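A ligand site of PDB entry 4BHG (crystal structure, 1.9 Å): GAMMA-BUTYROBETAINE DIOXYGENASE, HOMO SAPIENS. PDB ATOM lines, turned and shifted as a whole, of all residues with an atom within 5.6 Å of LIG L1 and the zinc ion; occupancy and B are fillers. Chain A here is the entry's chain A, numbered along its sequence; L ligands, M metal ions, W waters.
The side-chain carboxylate (OD2) of Asp 204 lies within hydrogen-bond range of a nitrogen (N1) of LIG L1 (3.4 Å).
An oxygen (O2) of LIG L1 is in hydrogen-bond range of the side-chain amide nitrogen (ND2) of Asn 292 (2.8 Å).
The backbone NH of Tyr 205 lies within hydrogen-bond range of an oxygen (O2) of LIG L1, at 2.9 Å.
The side-chain amide nitrogen (ND2) of Asn 191 is in hydrogen-bond range of an oxygen (O1) of LIG L1 (2.9 Å).
The side-chain hydroxyl (OH) of Tyr 366 lies close to a nitrogen (N1) of LIG L1, 3.4 Å away.
OD2 of Asp 204 sits at hydrogen-bond distance from OH of Tyr 366 (2.4 Å).
The side-chain amide nitrogen (NE2) of Gln 215 sits close to the side-chain carboxylate (OD2) of Asp 204, 3.3 Å away.
The side-chain hydroxyl (OH) of Tyr 177 sits at hydrogen-bond distance from the side-chain amide nitrogen (ND2) of Asn 191 (3.0 Å).
N of Ala 193 sits at hydrogen-bond distance from OD1 of Asn 191 (2.9 Å).
The backbone NH of Tyr 177 sits close to the side-chain hydroxyl of Thr 175.
OH of Tyr 177 lies within hydrogen-bond range of OD2 of Asp 261, 2.6 Å away.
Merely in contact with LIG L1: Tyr 177 (3.1 Å), Trp 181 (3.5 Å), Ala 193 (3.9 Å), Tyr 194 (3.5 Å), Pro 206 (3.9 Å) and Thr 295 (3.9 Å).
Hydrophobic or aromatic side chains within 4 Å of LIG L1: Tyr 177, Trp 181, Ala 193, Tyr 194, Tyr 205 and Pro 206.
Of the 19 residues printed, 11 come within 4 Å of LIG L1.
The nearest printed residue that does not touch LIG L1 is Thr 203 (4.3 Å).
OE1 of Gln 215 touches the zinc ion, at 3.9 Å.
Four residues have an atom within 4 Å of the zinc ion: His 202, Asp 204, Gln 215 and His 347.
The zinc ion is bound by an oxygen (O2) of LG2 L2 (1.9 Å), the side-chain carboxylate of Asp 204 (2.1 Å), a ring nitrogen (NE2) of His 347 (2.1 Å), an oxygen (O3) of LG2 L2 (2.2 Å) and a ring nitrogen (NE2) of His 202 (2.2 Å).
Water W4 lies within hydrogen-bond range of an oxygen (O1) of LIG L1 (2.8 Å), the side-chain amide oxygen (OD1) of Asn 191 (2.9 Å) and the side-chain amide nitrogen (ND2) of Asn 292 (3.2 Å).
Water W3 bridges the side-chain hydroxyl (OG1) of Thr 295 (2.9 Å) and an oxygen (O2) of LIG L1 (3.0 Å).
Water W2 bridges OD2 of Asp 261 and O1 of LIG L1.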
ATOM      1  N   THR A 175     -31.175 -14.168 -26.769  1.00  0.00           N
ATOM      2  CA  THR A 175     -30.858 -15.596 -26.656  1.00  0.00           C
ATOM      3  C   THR A 175     -31.841 -16.251 -25.669  1.00  0.00           C
ATOM      4  O   THR A 175     -32.685 -15.576 -25.048  1.00  0.00           O
ATOM      5  CB  THR A 175     -29.434 -15.842 -26.121  1.00  0.00           C
ATOM      6  OG1 THR A 175     -29.312 -15.396 -24.751  1.00  0.00           O
ATOM      7  CG2 THR A 175     -28.406 -15.148 -26.993  1.00  0.00           C
ATOM      8  N   TYR A 177     -31.330 -16.968 -22.745  1.00  0.00           N
ATOM      9  CA  TYR A 177     -31.179 -16.386 -21.415  1.00  0.00           C
ATOM     10  C   TYR A 177     -31.825 -15.018 -21.244  1.00  0.00           C
ATOM     11  O   TYR A 177     -31.799 -14.455 -20.133  1.00  0.00           O
ATOM     12  CB  TYR A 177     -29.699 -16.360 -20.994  1.00  0.00           C
ATOM     13  CG  TYR A 177     -29.135 -17.744 -20.753  1.00  0.00           C
ATOM     14  CD1 TYR A 177     -29.288 -18.383 -19.519  1.00  0.00           C
ATOM     15  CD2 TYR A 177     -28.491 -18.459 -21.770  1.00  0.00           C
ATOM     16  CE1 TYR A 177     -28.814 -19.675 -19.300  1.00  0.00           C
ATOM     17  CE2 TYR A 177     -28.026 -19.749 -21.568  1.00  0.00           C
ATOM     18  CZ  TYR A 177     -28.180 -20.350 -20.309  1.00  0.00           C
ATOM     19  OH  TYR A 177     -27.695 -21.628 -20.049  1.00  0.00           O
ATOM     20  N   TRP A 181     -29.864 -10.261 -18.931  1.00  0.00           N
ATOM     21  CA  TRP A 181     -29.864 -11.357 -17.945  1.00  0.00           C
ATOM     22  C   TRP A 181     -29.073 -10.937 -16.725  1.00  0.00           C
ATOM     23  O   TRP A 181     -28.204 -10.053 -16.790  1.00  0.00           O
ATOM     24  CB  TRP A 181     -29.313 -12.652 -18.541  1.00  0.00           C
ATOM     25  CG  TRP A 181     -28.386 -12.473 -19.695  1.00  0.00           C
ATOM     26  CD1 TRP A 181     -28.718 -12.497 -21.029  1.00  0.00           C
ATOM     27  CD2 TRP A 181     -26.963 -12.244 -19.652  1.00  0.00           C
ATOM     28  NE1 TRP A 181     -27.612 -12.274 -21.796  1.00  0.00           N
ATOM     29  CE2 TRP A 181     -26.528 -12.112 -20.980  1.00  0.00           C
ATOM     30  CE3 TRP A 181     -26.039 -12.113 -18.620  1.00  0.00           C
ATOM     31  CZ2 TRP A 181     -25.199 -11.888 -21.310  1.00  0.00           C
ATOM     32  CZ3 TRP A 181     -24.718 -11.894 -18.946  1.00  0.00           C
ATOM     33  CH2 TRP A 181     -24.310 -11.757 -20.294  1.00  0.00           C
ATOM     34  N   VAL A 183     -26.613 -11.811 -13.647  1.00  0.00           N
ATOM     35  CA  VAL A 183     -25.572 -12.681 -13.139  1.00  0.00           C
ATOM     36  C   VAL A 183     -25.561 -12.522 -11.626  1.00  0.00           C
ATOM     37  O   VAL A 183     -25.092 -11.513 -11.110  1.00  0.00           O
ATOM     38  CB  VAL A 183     -24.172 -12.364 -13.720  1.00  0.00           C
ATOM     39  CG1 VAL A 183     -23.160 -13.421 -13.292  1.00  0.00           C
ATOM     40  CG2 VAL A 183     -24.226 -12.237 -15.234  1.00  0.00           C
ATOM     41  N   ASN A 191     -27.102 -22.555 -15.023  1.00  0.00           N
ATOM     42  CA  ASN A 191     -25.841 -22.224 -15.675  1.00  0.00           C
ATOM     43  C   ASN A 191     -24.826 -21.951 -14.581  1.00  0.00           C
ATOM     44  O   ASN A 191     -25.171 -21.314 -13.577  1.00  0.00           O
ATOM     45  CB  ASN A 191     -26.029 -20.962 -16.541  1.00  0.00           C
ATOM     46  CG  ASN A 191     -24.852 -20.697 -17.449  1.00  0.00           C
ATOM     47  OD1 ASN A 191     -23.800 -20.272 -17.008  1.00  0.00           O
ATOM     48  ND2 ASN A 191     -25.046 -20.954 -18.729  1.00  0.00           N
ATOM     49  N   ALA A 193     -22.578 -19.828 -14.418  1.00  0.00           N
ATOM     50  CA  ALA A 193     -22.385 -18.414 -14.198  1.00  0.00           C
ATOM     51  C   ALA A 193     -23.308 -17.863 -13.094  1.00  0.00           C
ATOM     52  O   ALA A 193     -22.957 -16.869 -12.443  1.00  0.00           O
ATOM     53  CB  ALA A 193     -22.583 -17.654 -15.512  1.00  0.00           C
ATOM     54  N   TYR A 194     -24.441 -18.522 -12.851  1.00  0.00           N
ATOM     55  CA  TYR A 194     -25.432 -18.084 -11.855  1.00  0.00           C
ATOM     56  C   TYR A 194     -25.205 -18.798 -10.496  1.00  0.00           C
ATOM     57  O   TYR A 194     -26.156 -19.231  -9.843  1.00  0.00           O
ATOM     58  CB  TYR A 194     -26.838 -18.372 -12.361  1.00  0.00           C
ATOM     59  CG  TYR A 194     -27.188 -17.656 -13.673  1.00  0.00           C
ATOM     60  CD1 TYR A 194     -26.586 -16.418 -14.009  1.00  0.00           C
ATOM     61  CD2 TYR A 194     -28.159 -18.165 -14.511  1.00  0.00           C
ATOM     62  CE1 TYR A 194     -26.928 -15.762 -15.180  1.00  0.00           C
ATOM     63  CE2 TYR A 194     -28.504 -17.509 -15.716  1.00  0.00           C
ATOM     64  CZ  TYR A 194     -27.910 -16.290 -16.014  1.00  0.00           C
ATOM     65  OH  TYR A 194     -28.227 -15.624 -17.175  1.00  0.00           O
ATOM     66  N   LEU A 199     -15.277 -18.779 -12.541  1.00  0.00           N
ATOM     67  CA  LEU A 199     -15.373 -19.080 -13.949  1.00  0.00           C
ATOM     68  C   LEU A 199     -13.963 -18.960 -14.494  1.00  0.00           C
ATOM     69  O   LEU A 199     -13.348 -17.870 -14.411  1.00  0.00           O
ATOM     70  CB  LEU A 199     -16.317 -18.084 -14.663  1.00  0.00           C
ATOM     71  CG  LEU A 199     -17.759 -18.038 -14.133  1.00  0.00           C
ATOM     72  CD1 LEU A 199     -18.582 -17.015 -14.912  1.00  0.00           C
ATOM     73  CD2 LEU A 199     -18.400 -19.411 -14.188  1.00  0.00           C
ATOM     74  N   HIS A 202     -13.173 -18.298 -20.470  1.00  0.00           N
ATOM     75  CA  HIS A 202     -14.079 -18.839 -21.485  1.00  0.00           C
ATOM     76  C   HIS A 202     -14.546 -17.733 -22.413  1.00  0.00           C
ATOM     77  O   HIS A 202     -14.377 -16.541 -22.105  1.00  0.00           O
ATOM     78  CB  HIS A 202     -15.283 -19.481 -20.810  1.00  0.00           C
ATOM     79  CG  HIS A 202     -16.104 -18.518 -20.007  1.00  0.00           C
ATOM     80  ND1 HIS A 202     -15.692 -18.018 -18.796  1.00  0.00           N
ATOM     81  CD2 HIS A 202     -17.287 -17.928 -20.271  1.00  0.00           C
ATOM     82  CE1 HIS A 202     -16.593 -17.171 -18.337  1.00  0.00           C
ATOM     83  NE2 HIS A 202     -17.567 -17.094 -19.232  1.00  0.00           N
ATOM     84  N   THR A 203     -15.118 -18.141 -23.549  1.00  0.00           N
ATOM     85  CA  THR A 203     -15.968 -17.294 -24.339  1.00  0.00           C
ATOM     86  C   THR A 203     -17.423 -17.673 -24.053  1.00  0.00           C
ATOM     87  O   THR A 203     -17.722 -18.802 -23.650  1.00  0.00           O
ATOM     88  CB  THR A 203     -15.690 -17.442 -25.865  1.00  0.00           C
ATOM     89  OG1 THR A 203     -15.921 -18.800 -26.289  1.00  0.00           O
ATOM     90  CG2 THR A 203     -14.266 -17.044 -26.212  1.00  0.00           C
ATOM     91  N   ASP A 204     -18.332 -16.720 -24.215  1.00  0.00           N
ATOM     92  CA  ASP A 204     -19.733 -16.966 -23.926  1.00  0.00           C
ATOM     93  C   ASP A 204     -20.402 -17.624 -25.131  1.00  0.00           C
ATOM     94  O   ASP A 204     -20.230 -17.202 -26.265  1.00  0.00           O
ATOM     95  CB  ASP A 204     -20.487 -15.688 -23.597  1.00  0.00           C
ATOM     96  CG  ASP A 204     -20.564 -15.429 -22.095  1.00  0.00           C
ATOM     97  OD1 ASP A 204     -19.592 -15.743 -21.425  1.00  0.00           O
ATOM     98  OD2 ASP A 204     -21.612 -14.933 -21.626  1.00  0.00           O
ATOM     99  N   TYR A 205     -21.187 -18.660 -24.825  1.00  0.00           N
ATOM    100  CA  TYR A 205     -22.159 -19.230 -25.725  1.00  0.00           C
ATOM    101  C   TYR A 205     -21.609 -19.977 -26.945  1.00  0.00           C
ATOM    102  O   TYR A 205     -22.218 -19.901 -28.035  1.00  0.00           O
ATOM    103  CB  TYR A 205     -23.202 -18.164 -26.124  1.00  0.00           C
ATOM    104  CG  TYR A 205     -24.657 -18.498 -25.801  1.00  0.00           C
ATOM    105  CD1 TYR A 205     -25.162 -19.788 -25.892  1.00  0.00           C
ATOM    106  CD2 TYR A 205     -25.540 -17.504 -25.363  1.00  0.00           C
ATOM    107  CE1 TYR A 205     -26.483 -20.074 -25.607  1.00  0.00           C
ATOM    108  CE2 TYR A 205     -26.856 -17.783 -25.057  1.00  0.00           C
ATOM    109  CZ  TYR A 205     -27.332 -19.076 -25.199  1.00  0.00           C
ATOM    110  OH  TYR A 205     -28.640 -19.380 -24.911  1.00  0.00           O
ATOM    111  N   PRO A 206     -20.547 -20.790 -26.757  1.00  0.00           N
ATOM    112  CA  PRO A 206     -20.171 -21.680 -27.866  1.00  0.00           C
ATOM    113  C   PRO A 206     -21.203 -22.751 -28.196  1.00  0.00           C
ATOM    114  O   PRO A 206     -21.134 -23.392 -29.252  1.00  0.00           O
ATOM    115  CB  PRO A 206     -18.831 -22.274 -27.403  1.00  0.00           C
ATOM    116  CG  PRO A 206     -18.928 -22.235 -25.906  1.00  0.00           C
ATOM    117  CD  PRO A 206     -19.611 -20.926 -25.627  1.00  0.00           C
ATOM    118  N   GLN A 215     -20.105  -8.645 -25.912  1.00  0.00           N
ATOM    119  CA  GLN A 215     -20.777  -8.835 -24.661  1.00  0.00           C
ATOM    120  C   GLN A 215     -20.701  -7.558 -23.846  1.00  0.00           C
ATOM    121  O   GLN A 215     -19.678  -6.881 -23.841  1.00  0.00           O
ATOM    122  CB  GLN A 215     -20.140 -10.005 -23.903  1.00  0.00           C
ATOM    123  CG  GLN A 215     -20.829 -10.376 -22.600  1.00  0.00           C
ATOM    124  CD  GLN A 215     -20.313 -11.679 -22.002  1.00  0.00           C
ATOM    125  OE1 GLN A 215     -20.413 -11.931 -20.780  1.00  0.00           O
ATOM    126  NE2 GLN A 215     -19.758 -12.524 -22.853  1.00  0.00           N
ATOM    127  N   ASP A 261     -26.179 -27.143 -24.164  1.00  0.00           N
ATOM    128  CA  ASP A 261     -26.839 -26.379 -23.111  1.00  0.00           C
ATOM    129  C   ASP A 261     -28.299 -26.792 -23.090  1.00  0.00           C
ATOM    130  O   ASP A 261     -29.000 -26.640 -24.098  1.00  0.00           O
ATOM    131  CB  ASP A 261     -26.729 -24.879 -23.401  1.00  0.00           C
ATOM    132  CG  ASP A 261     -26.933 -24.023 -22.184  1.00  0.00           C
ATOM    133  OD1 ASP A 261     -26.808 -24.529 -21.051  1.00  0.00           O
ATOM    134  OD2 ASP A 261     -27.209 -22.804 -22.348  1.00  0.00           O
ATOM    135  N   ASN A 292     -15.930 -22.732 -23.874  1.00  0.00           N
ATOM    136  CA  ASN A 292     -16.425 -22.614 -22.504  1.00  0.00           C
ATOM    137  C   ASN A 292     -16.384 -24.025 -21.923  1.00  0.00           C
ATOM    138  O   ASN A 292     -17.053 -24.927 -22.398  1.00  0.00           O
ATOM    139  CB  ASN A 292     -17.836 -22.070 -22.447  1.00  0.00           C
ATOM    140  CG  ASN A 292     -18.307 -21.796 -21.021  1.00  0.00           C
ATOM    141  OD1 ASN A 292     -17.742 -22.318 -20.034  1.00  0.00           O
ATOM    142  ND2 ASN A 292     -19.355 -20.984 -20.896  1.00  0.00           N
ATOM    143  N   THR A 295     -19.693 -25.770 -20.767  1.00  0.00           N
ATOM    144  CA  THR A 295     -20.697 -26.220 -21.719  1.00  0.00           C
ATOM    145  C   THR A 295     -20.131 -27.144 -22.790  1.00  0.00           C
ATOM    146  O   THR A 295     -20.879 -27.627 -23.648  1.00  0.00           O
ATOM    147  CB  THR A 295     -21.402 -25.022 -22.391  1.00  0.00           C
ATOM    148  OG1 THR A 295     -20.473 -24.279 -23.180  1.00  0.00           O
ATOM    149  CG2 THR A 295     -22.031 -24.098 -21.342  1.00  0.00           C
ATOM    150  N   HIS A 347     -12.739 -14.447 -20.945  1.00  0.00           N
ATOM    151  CA  HIS A 347     -12.950 -13.763 -19.691  1.00  0.00           C
ATOM    152  C   HIS A 347     -13.262 -14.764 -18.591  1.00  0.00           C
ATOM    153  O   HIS A 347     -13.609 -15.946 -18.821  1.00  0.00           O
ATOM    154  CB  HIS A 347     -14.044 -12.700 -19.831  1.00  0.00           C
ATOM    155  CG  HIS A 347     -15.403 -13.251 -20.165  1.00  0.00           C
ATOM    156  ND1 HIS A 347     -15.736 -13.664 -21.437  1.00  0.00           N
ATOM    157  CD2 HIS A 347     -16.500 -13.441 -19.411  1.00  0.00           C
ATOM    158  CE1 HIS A 347     -16.979 -14.109 -21.449  1.00  0.00           C
ATOM    159  NE2 HIS A 347     -17.469 -14.007 -20.221  1.00  0.00           N
ATOM    160  N   TYR A 366     -25.885  -9.217 -25.031  1.00  0.00           N
ATOM    161  CA  TYR A 366     -25.053  -9.503 -26.179  1.00  0.00           C
ATOM    162  C   TYR A 366     -25.450  -8.615 -27.347  1.00  0.00           C
ATOM    163  O   TYR A 366     -26.578  -8.145 -27.434  1.00  0.00           O
ATOM    164  CB  TYR A 366     -25.258 -10.962 -26.614  1.00  0.00           C
ATOM    165  CG  TYR A 366     -24.858 -11.995 -25.562  1.00  0.00           C
ATOM    166  CD1 TYR A 366     -23.560 -12.023 -25.054  1.00  0.00           C
ATOM    167  CD2 TYR A 366     -25.753 -12.970 -25.155  1.00  0.00           C
ATOM    168  CE1 TYR A 366     -23.190 -12.975 -24.105  1.00  0.00           C
ATOM    169  CE2 TYR A 366     -25.378 -13.948 -24.258  1.00  0.00           C
ATOM    170  CZ  TYR A 366     -24.085 -13.946 -23.744  1.00  0.00           C
ATOM    171  OH  TYR A 366     -23.749 -14.919 -22.813  1.00  0.00           O
HETATM  172  C1  LIG L   1     -22.623 -19.745 -21.787  1.00  0.00           C
HETATM  173  N1  LIG L   1     -23.884 -17.106 -20.271  1.00  0.00           N
HETATM  174  O1  LIG L   1     -23.155 -20.414 -20.870  1.00  0.00           O
HETATM  175  C2  LIG L   1     -23.250 -18.460 -22.265  1.00  0.00           C
HETATM  176  N2  LIG L   1     -24.750 -16.426 -19.373  1.00  0.00           N
HETATM  177  O2  LIG L   1     -21.613 -20.129 -22.386  1.00  0.00           O
HETATM  178  C3  LIG L   1     -24.381 -17.908 -21.388  1.00  0.00           C
HETATM  179  C4  LIG L   1     -23.975 -15.569 -18.466  1.00  0.00           C
HETATM  180  C5  LIG L   1     -25.528 -17.369 -18.535  1.00  0.00           C
HETATM  181  C6  LIG L   1     -25.532 -15.385 -20.047  1.00  0.00           C
HETATM  182  C7  LIG L   1     -26.599 -15.880 -20.899  1.00  0.00           C
HETATM  183  C1  LG2 L   2     -20.715 -14.934 -17.506  1.00  0.00           C
HETATM  184  C2  LG2 L   2     -19.499 -14.337 -16.948  1.00  0.00           C
HETATM  185  C3  LG2 L   2     -18.534 -12.774 -15.346  1.00  0.00           C
HETATM  186  C4  LG2 L   2     -18.720 -12.361 -13.897  1.00  0.00           C
HETATM  187  O1  LG2 L   2     -21.760 -14.747 -16.833  1.00  0.00           O
HETATM  188  O2  LG2 L   2     -20.642 -15.543 -18.641  1.00  0.00           O
HETATM  189  O3  LG2 L   2     -18.446 -14.499 -17.544  1.00  0.00           O
HETATM  190  O4  LG2 L   2     -17.883 -11.586 -13.423  1.00  0.00           O
HETATM  191  N1  LG2 L   2     -19.629 -13.600 -15.851  1.00  0.00           N
HETATM  192  O5  LG2 L   2     -19.664 -12.832 -13.228  1.00  0.00           O
HETATM  193 ZN    ZN M   1     -18.921 -15.331 -19.516  1.00  0.00          ZN
HETATM  194  O   HOH W   1     -21.198 -18.213 -19.456  1.00  0.00           O
HETATM  195  O   HOH W   2     -24.609 -21.935 -23.011  1.00  0.00           O
HETATM  196  O   HOH W   3     -22.303 -22.285 -24.340  1.00  0.00           O
HETATM  197  O   HOH W   4     -21.670 -21.354 -18.651  1.00  0.00           O
